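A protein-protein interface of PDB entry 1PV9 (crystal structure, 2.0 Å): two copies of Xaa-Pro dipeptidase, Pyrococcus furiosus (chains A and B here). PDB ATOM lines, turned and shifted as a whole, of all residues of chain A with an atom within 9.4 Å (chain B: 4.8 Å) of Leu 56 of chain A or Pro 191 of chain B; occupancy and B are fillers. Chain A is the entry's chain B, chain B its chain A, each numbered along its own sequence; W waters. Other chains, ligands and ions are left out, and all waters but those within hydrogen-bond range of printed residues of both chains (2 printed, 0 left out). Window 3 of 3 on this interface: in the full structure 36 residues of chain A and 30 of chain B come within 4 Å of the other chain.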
ATOM      1  N   PRO A  36     -18.819  17.449  -3.216  1.00  0.00           N
ATOM      2  CA  PRO A  36     -20.126  17.829  -3.769  1.00  0.00           C
ATOM      3  C   PRO A  36     -19.990  18.901  -4.852  1.00  0.00           C
ATOM      4  O   PRO A  36     -19.370  19.943  -4.617  1.00  0.00           O
ATOM      5  CB  PRO A  36     -20.881  18.373  -2.550  1.00  0.00           C
ATOM      6  CG  PRO A  36     -20.046  17.991  -1.361  1.00  0.00           C
ATOM      7  CD  PRO A  36     -18.635  17.966  -1.848  1.00  0.00           C
ATOM      8  N   LEU A  37     -20.562  18.628  -6.021  1.00  0.00           N
ATOM      9  CA  LEU A  37     -20.485  19.522  -7.178  1.00  0.00           C
ATOM     10  C   LEU A  37     -21.119  20.894  -6.922  1.00  0.00           C
ATOM     11  O   LEU A  37     -20.540  21.925  -7.275  1.00  0.00           O
ATOM     12  CB  LEU A  37     -21.123  18.849  -8.402  1.00  0.00           C
ATOM     13  CG  LEU A  37     -21.003  19.511  -9.779  1.00  0.00           C
ATOM     14  CD1 LEU A  37     -19.679  19.167 -10.450  1.00  0.00           C
ATOM     15  CD2 LEU A  37     -22.167  19.096 -10.660  1.00  0.00           C
ATOM     16  N   GLY A  38     -22.295  20.896  -6.299  1.00  0.00           N
ATOM     17  CA  GLY A  38     -23.048  22.116  -6.052  1.00  0.00           C
ATOM     18  C   GLY A  38     -22.607  22.889  -4.823  1.00  0.00           C
ATOM     19  O   GLY A  38     -23.296  23.811  -4.380  1.00  0.00           O
ATOM     20  N   GLY A  39     -21.457  22.515  -4.273  1.00  0.00           N
ATOM     21  CA  GLY A  39     -20.918  23.173  -3.101  1.00  0.00           C
ATOM     22  C   GLY A  39     -20.758  22.222  -1.935  1.00  0.00           C
ATOM     23  O   GLY A  39     -21.645  21.421  -1.643  1.00  0.00           O
ATOM     24  N   GLY A  40     -19.599  22.305  -1.292  1.00  0.00           N
ATOM     25  CA  GLY A  40     -19.309  21.576  -0.071  1.00  0.00           C
ATOM     26  C   GLY A  40     -18.338  22.420   0.725  1.00  0.00           C
ATOM     27  O   GLY A  40     -17.414  22.999   0.156  1.00  0.00           O
ATOM     28  N   TYR A  41     -18.553  22.512   2.033  1.00  0.00           N
ATOM     29  CA  TYR A  41     -17.769  23.411   2.872  1.00  0.00           C
ATOM     30  C   TYR A  41     -17.487  22.765   4.223  1.00  0.00           C
ATOM     31  O   TYR A  41     -18.405  22.283   4.886  1.00  0.00           O
ATOM     32  CB  TYR A  41     -18.493  24.761   3.041  1.00  0.00           C
ATOM     33  CG  TYR A  41     -19.063  25.319   1.747  1.00  0.00           C
ATOM     34  CD1 TYR A  41     -20.368  25.013   1.343  1.00  0.00           C
ATOM     35  CD2 TYR A  41     -18.293  26.133   0.916  1.00  0.00           C
ATOM     36  CE1 TYR A  41     -20.889  25.507   0.144  1.00  0.00           C
ATOM     37  CE2 TYR A  41     -18.805  26.634  -0.280  1.00  0.00           C
ATOM     38  CZ  TYR A  41     -20.102  26.317  -0.658  1.00  0.00           C
ATOM     39  OH  TYR A  41     -20.613  26.814  -1.837  1.00  0.00           O
ATOM     40  N   VAL A  53     -23.318  21.196   3.378  1.00  0.00           N
ATOM     41  CA  VAL A  53     -23.720  21.058   1.980  1.00  0.00           C
ATOM     42  C   VAL A  53     -25.122  21.633   1.762  1.00  0.00           C
ATOM     43  O   VAL A  53     -25.927  21.649   2.690  1.00  0.00           O
ATOM     44  CB  VAL A  53     -23.675  19.571   1.507  1.00  0.00           C
ATOM     45  CG1 VAL A  53     -22.245  19.029   1.521  1.00  0.00           C
ATOM     46  CG2 VAL A  53     -24.601  18.689   2.347  1.00  0.00           C
ATOM     47  N   PRO A  54     -25.416  22.124   0.556  1.00  0.00           N
ATOM     48  CA  PRO A  54     -26.798  22.468   0.196  1.00  0.00           C
ATOM     49  C   PRO A  54     -27.659  21.204   0.169  1.00  0.00           C
ATOM     50  O   PRO A  54     -27.119  20.109  -0.009  1.00  0.00           O
ATOM     51  CB  PRO A  54     -26.662  23.061  -1.209  1.00  0.00           C
ATOM     52  CG  PRO A  54     -25.360  22.551  -1.727  1.00  0.00           C
ATOM     53  CD  PRO A  54     -24.473  22.411  -0.542  1.00  0.00           C
ATOM     54  N   GLU A  55     -28.970  21.348   0.351  1.00  0.00           N
ATOM     55  CA  GLU A  55     -29.854  20.180   0.446  1.00  0.00           C
ATOM     56  C   GLU A  55     -29.842  19.289  -0.800  1.00  0.00           C
ATOM     57  O   GLU A  55     -30.104  18.092  -0.705  1.00  0.00           O
ATOM     58  CB  GLU A  55     -31.286  20.569   0.848  1.00  0.00           C
ATOM     59  CG  GLU A  55     -31.921  21.700   0.056  1.00  0.00           C
ATOM     60  CD  GLU A  55     -33.310  22.058   0.560  1.00  0.00           C
ATOM     61  OE1 GLU A  55     -33.451  22.397   1.754  1.00  0.00           O
ATOM     62  OE2 GLU A  55     -34.267  21.997  -0.241  1.00  0.00           O
ATOM     63  N   LEU A  56     -29.508  19.868  -1.952  1.00  0.00           N
ATOM     64  CA  LEU A  56     -29.412  19.107  -3.197  1.00  0.00           C
ATOM     65  C   LEU A  56     -28.201  18.167  -3.222  1.00  0.00           C
ATOM     66  O   LEU A  56     -28.138  17.252  -4.044  1.00  0.00           O
ATOM     67  CB  LEU A  56     -29.439  20.044  -4.416  1.00  0.00           C
ATOM     68  CG  LEU A  56     -28.165  20.398  -5.190  1.00  0.00           C
ATOM     69  CD1 LEU A  56     -28.481  20.564  -6.665  1.00  0.00           C
ATOM     70  CD2 LEU A  56     -27.535  21.661  -4.637  1.00  0.00           C
ATOM     71  N   GLU A  57     -27.253  18.390  -2.312  1.00  0.00           N
ATOM     72  CA  GLU A  57     -26.065  17.542  -2.201  1.00  0.00           C
ATOM     73  C   GLU A  57     -26.062  16.670  -0.940  1.00  0.00           C
ATOM     74  O   GLU A  57     -25.157  15.855  -0.746  1.00  0.00           O
ATOM     75  CB  GLU A  57     -24.787  18.390  -2.255  1.00  0.00           C
ATOM     76  CG  GLU A  57     -24.567  19.121  -3.575  1.00  0.00           C
ATOM     77  CD  GLU A  57     -24.078  18.221  -4.704  1.00  0.00           C
ATOM     78  OE1 GLU A  57     -24.103  16.978  -4.571  1.00  0.00           O
ATOM     79  OE2 GLU A  57     -23.668  18.767  -5.747  1.00  0.00           O
ATOM     80  N   TYR A  58     -27.080  16.835  -0.100  1.00  0.00           N
ATOM     81  CA  TYR A  58     -27.114  16.198   1.217  1.00  0.00           C
ATOM     82  C   TYR A  58     -26.966  14.679   1.156  1.00  0.00           C
ATOM     83  O   TYR A  58     -26.045  14.119   1.749  1.00  0.00           O
ATOM     84  CB  TYR A  58     -28.381  16.594   1.983  1.00  0.00           C
ATOM     85  CG  TYR A  58     -28.437  16.062   3.401  1.00  0.00           C
ATOM     86  CD1 TYR A  58     -27.474  16.425   4.344  1.00  0.00           C
ATOM     87  CD2 TYR A  58     -29.454  15.194   3.797  1.00  0.00           C
ATOM     88  CE1 TYR A  58     -27.524  15.941   5.648  1.00  0.00           C
ATOM     89  CE2 TYR A  58     -29.513  14.701   5.100  1.00  0.00           C
ATOM     90  CZ  TYR A  58     -28.545  15.079   6.018  1.00  0.00           C
ATOM     91  OH  TYR A  58     -28.593  14.597   7.305  1.00  0.00           O
ATOM     92  N   GLU A  59     -27.860  14.024   0.416  1.00  0.00           N
ATOM     93  CA  GLU A  59     -27.882  12.562   0.337  1.00  0.00           C
ATOM     94  C   GLU A  59     -26.576  11.950  -0.182  1.00  0.00           C
ATOM     95  O   GLU A  59     -26.098  10.958   0.370  1.00  0.00           O
ATOM     96  CB  GLU A  59     -29.074  12.081  -0.497  1.00  0.00           C
ATOM     97  CG  GLU A  59     -30.419  12.208   0.208  1.00  0.00           C
ATOM     98  CD  GLU A  59     -30.530  11.340   1.452  1.00  0.00           C
ATOM     99  OE1 GLU A  59     -30.141  10.152   1.402  1.00  0.00           O
ATOM    100  OE2 GLU A  59     -31.014  11.849   2.482  1.00  0.00           O
ATOM    101  N   MET A  60     -26.001  12.545  -1.228  1.00  0.00           N
ATOM    102  CA  MET A  60     -24.749  12.047  -1.801  1.00  0.00           C
ATOM    103  C   MET A  60     -23.569  12.213  -0.845  1.00  0.00           C
ATOM    104  O   MET A  60     -22.744  11.305  -0.708  1.00  0.00           O
ATOM    105  CB  MET A  60     -24.445  12.716  -3.144  1.00  0.00           C
ATOM    106  CG  MET A  60     -24.321  11.725  -4.301  1.00  0.00           C
ATOM    107  SD  MET A  60     -23.447  12.329  -5.776  1.00  0.00           S
ATOM    108  CE  MET A  60     -24.252  13.888  -6.042  1.00  0.00           C
ATOM    109  N   ALA A  61     -23.503  13.369  -0.186  1.00  0.00           N
ATOM    110  CA  ALA A  61     -22.465  13.649   0.806  1.00  0.00           C
ATOM    111  C   ALA A  61     -22.574  12.747   2.036  1.00  0.00           C
ATOM    112  O   ALA A  61     -21.560  12.389   2.632  1.00  0.00           O
ATOM    113  CB  ALA A  61     -22.503  15.116   1.217  1.00  0.00           C
ATOM    114  N   LYS A  62     -23.802  12.383   2.400  1.00  0.00           N
ATOM    115  CA  LYS A  62     -24.068  11.559   3.584  1.00  0.00           C
ATOM    116  C   LYS A  62     -23.513  10.135   3.483  1.00  0.00           C
ATOM    117  O   LYS A  62     -23.085   9.560   4.487  1.00  0.00           O
ATOM    118  CB  LYS A  62     -25.573  11.507   3.869  1.00  0.00           C
ATOM    119  CG  LYS A  62     -25.928  11.417   5.344  1.00  0.00           C
ATOM    120  CD  LYS A  62     -27.414  11.657   5.564  1.00  0.00           C
ATOM    121  CE  LYS A  62     -27.976  10.723   6.622  1.00  0.00           C
ATOM    122  NZ  LYS A  62     -28.365   9.401   6.056  1.00  0.00           N
ATOM    123  N   VAL A  70     -24.084  18.250   7.657  1.00  0.00           N
ATOM    124  CA  VAL A  70     -25.295  19.034   7.905  1.00  0.00           C
ATOM    125  C   VAL A  70     -25.669  19.863   6.675  1.00  0.00           C
ATOM    126  O   VAL A  70     -24.812  20.500   6.049  1.00  0.00           O
ATOM    127  CB  VAL A  70     -25.237  19.888   9.234  1.00  0.00           C
ATOM    128  CG1 VAL A  70     -23.874  19.794   9.924  1.00  0.00           C
ATOM    129  CG2 VAL A  70     -25.655  21.345   9.010  1.00  0.00           C
ATOM    130  N   LYS A  71     -26.948  19.822   6.316  1.00  0.00           N
ATOM    131  CA  LYS A  71     -27.427  20.575   5.164  1.00  0.00           C
ATOM    132  C   LYS A  71     -27.877  21.979   5.550  1.00  0.00           C
ATOM    133  O   LYS A  71     -28.330  22.213   6.674  1.00  0.00           O
ATOM    134  CB  LYS A  71     -28.534  19.820   4.413  1.00  0.00           C
ATOM    135  CG  LYS A  71     -29.835  19.623   5.178  1.00  0.00           C
ATOM    136  CD  LYS A  71     -30.896  18.985   4.289  1.00  0.00           C
ATOM    137  CE  LYS A  71     -32.268  19.584   4.553  1.00  0.00           C
ATOM    138  NZ  LYS A  71     -33.326  18.936   3.728  1.00  0.00           N
ATOM    139  N   PHE A  72     -27.723  22.909   4.613  1.00  0.00           N
ATOM    140  CA  PHE A  72     -28.255  24.258   4.767  1.00  0.00           C
ATOM    141  C   PHE A  72     -29.201  24.584   3.617  1.00  0.00           C
ATOM    142  O   PHE A  72     -28.993  24.135   2.487  1.00  0.00           O
ATOM    143  CB  PHE A  72     -27.133  25.302   4.878  1.00  0.00           C
ATOM    144  CG  PHE A  72     -26.118  25.251   3.758  1.00  0.00           C
ATOM    145  CD1 PHE A  72     -26.370  25.869   2.534  1.00  0.00           C
ATOM    146  CD2 PHE A  72     -24.898  24.608   3.942  1.00  0.00           C
ATOM    147  CE1 PHE A  72     -25.430  25.830   1.502  1.00  0.00           C
ATOM    148  CE2 PHE A  72     -23.949  24.567   2.921  1.00  0.00           C
ATOM    149  CZ  PHE A  72     -24.216  25.178   1.699  1.00  0.00           C
ATOM    150  N   LYS A  73     -30.251  25.343   3.918  1.00  0.00           N
ATOM    151  CA  LYS A  73     -31.183  25.815   2.899  1.00  0.00           C
ATOM    152  C   LYS A  73     -30.596  27.041   2.207  1.00  0.00           C
ATOM    153  O   LYS A  73     -30.676  27.180   0.984  1.00  0.00           O
ATOM    154  CB  LYS A  73     -32.545  26.141   3.520  1.00  0.00           C
ATOM    155  CG  LYS A  73     -33.726  25.902   2.593  1.00  0.00           C
ATOM    156  CD  LYS A  73     -34.835  25.138   3.296  1.00  0.00           C
ATOM    157  CE  LYS A  73     -36.034  24.941   2.383  1.00  0.00           C
ATOM    158  NZ  LYS A  73     -36.037  23.591   1.754  1.00  0.00           N
ATOM    159  N   ILE B 181     -24.307  14.062 -16.380  1.00  0.00           N
ATOM    160  CA  ILE B 181     -25.067  13.296 -15.407  1.00  0.00           C
ATOM    161  C   ILE B 181     -25.885  12.225 -16.124  1.00  0.00           C
ATOM    162  O   ILE B 181     -26.766  12.531 -16.927  1.00  0.00           O
ATOM    163  CB  ILE B 181     -25.969  14.230 -14.550  1.00  0.00           C
ATOM    164  CG1 ILE B 181     -25.117  15.063 -13.582  1.00  0.00           C
ATOM    165  CG2 ILE B 181     -27.034  13.432 -13.785  1.00  0.00           C
ATOM    166  CD1 ILE B 181     -25.655  16.460 -13.333  1.00  0.00           C
ATOM    167  N   ALA B 189     -32.169   9.937  -7.687  1.00  0.00           N
ATOM    168  CA  ALA B 189     -32.583  10.738  -6.532  1.00  0.00           C
ATOM    169  C   ALA B 189     -31.538  11.792  -6.153  1.00  0.00           C
ATOM    170  O   ALA B 189     -31.801  12.670  -5.326  1.00  0.00           O
ATOM    171  CB  ALA B 189     -32.888   9.836  -5.342  1.00  0.00           C
ATOM    172  N   LEU B 190     -30.354  11.697  -6.756  1.00  0.00           N
ATOM    173  CA  LEU B 190     -29.298  12.688  -6.562  1.00  0.00           C
ATOM    174  C   LEU B 190     -29.254  13.650  -7.749  1.00  0.00           C
ATOM    175  O   LEU B 190     -28.926  13.241  -8.865  1.00  0.00           O
ATOM    176  CB  LEU B 190     -27.933  12.013  -6.366  1.00  0.00           C
ATOM    177  CG  LEU B 190     -27.887  10.593  -5.790  1.00  0.00           C
ATOM    178  CD1 LEU B 190     -26.648   9.862  -6.288  1.00  0.00           C
ATOM    179  CD2 LEU B 190     -27.938  10.608  -4.265  1.00  0.00           C
ATOM    180  N   PRO B 191     -29.601  14.917  -7.514  1.00  0.00           N
ATOM    181  CA  PRO B 191     -29.601  15.940  -8.572  1.00  0.00           C
ATOM    182  C   PRO B 191     -28.282  16.039  -9.343  1.00  0.00           C
ATOM    183  O   PRO B 191     -28.318  16.209 -10.562  1.00  0.00           O
ATOM    184  CB  PRO B 191     -29.863  17.235  -7.801  1.00  0.00           C
ATOM    185  CG  PRO B 191     -30.639  16.797  -6.608  1.00  0.00           C
ATOM    186  CD  PRO B 191     -30.047  15.471  -6.223  1.00  0.00           C
ATOM    187  N   HIS B 192     -27.151  15.931  -8.649  1.00  0.00           N
ATOM    188  CA  HIS B 192     -25.844  15.984  -9.302  1.00  0.00           C
ATOM    189  C   HIS B 192     -25.188  14.600  -9.397  1.00  0.00           C
ATOM    190  O   HIS B 192     -23.992  14.446  -9.141  1.00  0.00           O
ATOM    191  CB  HIS B 192     -24.926  16.998  -8.600  1.00  0.00           C
ATOM    192  CG  HIS B 192     -25.304  18.427  -8.851  1.00  0.00           C
ATOM    193  ND1 HIS B 192     -26.068  18.819  -9.931  1.00  0.00           N
ATOM    194  CD2 HIS B 192     -25.021  19.558  -8.163  1.00  0.00           C
ATOM    195  CE1 HIS B 192     -26.242  20.128  -9.894  1.00  0.00           C
ATOM    196  NE2 HIS B 192     -25.618  20.600  -8.831  1.00  0.00           N
ATOM    197  N   GLY B 193     -25.980  13.600  -9.781  1.00  0.00           N
ATOM    198  CA  GLY B 193     -25.495  12.237  -9.911  1.00  0.00           C
ATOM    199  C   GLY B 193     -24.690  11.988 -11.175  1.00  0.00           C
ATOM    200  O   GLY B 193     -25.144  11.284 -12.084  1.00  0.00           O
ATOM    201  N   ILE B 279     -35.807  19.872  -4.080  1.00  0.00           N
ATOM    202  CA  ILE B 279     -34.710  20.274  -3.190  1.00  0.00           C
ATOM    203  C   ILE B 279     -33.668  21.235  -3.784  1.00  0.00           C
ATOM    204  O   ILE B 279     -32.561  21.366  -3.252  1.00  0.00           O
ATOM    205  CB  ILE B 279     -34.017  19.014  -2.587  1.00  0.00           C
ATOM    206  CG1 ILE B 279     -33.555  18.059  -3.698  1.00  0.00           C
ATOM    207  CG2 ILE B 279     -34.952  18.317  -1.590  1.00  0.00           C
ATOM    208  CD1 ILE B 279     -32.611  16.952  -3.234  1.00  0.00           C
ATOM    209  N   HIS B 280     -34.022  21.897  -4.881  1.00  0.00           N
ATOM    210  CA  HIS B 280     -33.158  22.913  -5.480  1.00  0.00           C
ATOM    211  C   HIS B 280     -33.969  24.021  -6.148  1.00  0.00           C
ATOM    212  O   HIS B 280     -35.193  23.926  -6.267  1.00  0.00           O
ATOM    213  CB  HIS B 280     -32.159  22.288  -6.470  1.00  0.00           C
ATOM    214  CG  HIS B 280     -32.799  21.559  -7.611  1.00  0.00           C
ATOM    215  ND1 HIS B 280     -33.374  22.207  -8.684  1.00  0.00           N
ATOM    216  CD2 HIS B 280     -32.935  20.234  -7.858  1.00  0.00           C
ATOM    217  CE1 HIS B 280     -33.850  21.313  -9.532  1.00  0.00           C
ATOM    218  NE2 HIS B 280     -33.593  20.109  -9.057  1.00  0.00           N
ATOM    219  N   TYR B 317     -37.236  14.497  -6.007  1.00  0.00           N
ATOM    220  CA  TYR B 317     -36.219  13.518  -5.640  1.00  0.00           C
ATOM    221  C   TYR B 317     -36.585  12.790  -4.356  1.00  0.00           C
ATOM    222  O   TYR B 317     -36.635  13.389  -3.281  1.00  0.00           O
ATOM    223  CB  TYR B 317     -34.844  14.192  -5.512  1.00  0.00           C
ATOM    224  CG  TYR B 317     -34.513  15.067  -6.695  1.00  0.00           C
ATOM    225  CD1 TYR B 317     -34.861  16.416  -6.704  1.00  0.00           C
ATOM    226  CD2 TYR B 317     -33.878  14.539  -7.819  1.00  0.00           C
ATOM    227  CE1 TYR B 317     -34.576  17.220  -7.798  1.00  0.00           C
ATOM    228  CE2 TYR B 317     -33.589  15.334  -8.916  1.00  0.00           C
ATOM    229  CZ  TYR B 317     -33.938  16.672  -8.898  1.00  0.00           C
ATOM    230  OH  TYR B 317     -33.652  17.464  -9.983  1.00  0.00           O
ATOM    231  N   ARG B 325     -36.151  14.936 -13.344  1.00  0.00           N
ATOM    232  CA  ARG B 325     -35.877  16.333 -13.659  1.00  0.00           C
ATOM    233  C   ARG B 325     -36.054  16.540 -15.157  1.00  0.00           C
ATOM    234  O   ARG B 325     -35.661  15.689 -15.961  1.00  0.00           O
ATOM    235  CB  ARG B 325     -34.463  16.734 -13.214  1.00  0.00           C
ATOM    236  CG  ARG B 325     -34.061  18.174 -13.574  1.00  0.00           C
ATOM    237  CD  ARG B 325     -32.831  18.699 -12.833  1.00  0.00           C
ATOM    238  NE  ARG B 325     -31.588  18.056 -13.260  1.00  0.00           N
ATOM    239  CZ  ARG B 325     -30.967  17.087 -12.592  1.00  0.00           C
ATOM    240  NH1 ARG B 325     -31.466  16.624 -11.452  1.00  0.00           N
ATOM    241  NH2 ARG B 325     -29.840  16.575 -13.067  1.00  0.00           N
HETATM  242  O   HOH W   1     -30.216  22.735  -2.612  1.00  0.00           O
HETATM  243  O   HOH W   2     -26.769  15.651  -5.622  1.00  0.00           O
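Hydrophobic or aromatic side chains of chain B that line the printed part of chain A: Leu 190, Pro 191, His 192 and Ile 279. Hydrophobic or aromatic side chains of chain A within 4 Å of the printed part of chain B: Leu 37, Leu 56 and Met 60.
No position is printed for both chains. Of the 9 pairs that touch across the chains among the printed residues, none has its exchanged pair printed and touching as well.
The side-chain amino group (NZ) of Lys 71 of chain A is in salt-bridge range of the side-chain carboxylate (OE1) of Glu 55 of chain A (3.99 Å). The side-chain carboxylate of Glu 55 of chain A lies within salt-bridge range of the side-chain amino group of Lys 73 of chain A (2.8 Å). The backbone NH of Gly 38 of chain A sits at hydrogen-bond distance from the side-chain carboxylate of Glu 57 of chain A, 2.6 Å away. The side-chain carboxylate (OE2) of Glu 57 of chain A is in hydrogen-bond range of the backbone NH (N) of Leu 37 of chain A, 3.1 Å away. O of Pro 191 of chain B is in hydrogen-bond range of NH2 of Arg 325 of chain B, at 3.0 Å.
Water W2 lies within hydrogen-bond range of the backbone carbonyl oxygen (O) of Leu 56 of chain A, the backbone NH (N) of His 192 of chain B and the side-chain carboxylate (OE1) of Glu 57 of chain A. Water W1 bridges O of Ile 279 of chain B (2.8 Å) and N of Leu 56 of chain A (3.0 Å).
Leu 56 of chain A touches just these residues of chain B: Pro 191 (3.4 Å), His 192 (3.6 Å) and Ile 279 (3.6 Å). Of chain A, only Leu 56 (3.4 Å) comes within 4 Å of Pro 191 of chain B. His 192 of chain B touches just these residues of chain A: Leu 37 (3.7 Å), Gly 38 (3.6 Å), Leu 56 (3.6 Å), Glu 57 (2.9 Å) and Met 60 (3.2 Å). Of the printed residues of chain B, Glu 57 of chain A touches His 192. Printed residues of chain B within 4 Å of Met 60 of chain A: Leu 190 and His 192. Printed residues of chain B within 4 Å of Glu 55 of chain A: Ile 279. Printed residues of chain B within 4 Å of Gly 38 of chain A: His 192 (3.6 Å). Pro 36 of chain A touches none of the printed residues of chain B. The nearest printed residue of chain A that does not touch Pro 191 of chain B is Glu 57 of chain A (5.6 Å). The nearest printed residue of chain B that does not touch Gly 38 of chain A is Pro 191 of chain B (8.3 Å).
Among the printed residues, pairs that only touch across the chains: Leu 37 of chain A with His 192 of chain B (3.7 Å), Gly 38 of chain A with His 192 of chain B (3.6 Å), Glu 55 of chain A with Ile 279 of chain B (3.4 Å), Leu 56 of chain A with Pro 191 of chain B (3.4 Å), Leu 56 of chain A with His 192 of chain B (3.6 Å), Leu 56 of chain A with Ile 279 of chain B (3.6 Å), Glu 57 of chain A with His 192 of chain B (2.9 Å), Met 60 of chain A with Leu 190 of chain B (3.6 Å) and Met 60 of chain A with His 192 of chain B (3.2 Å).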
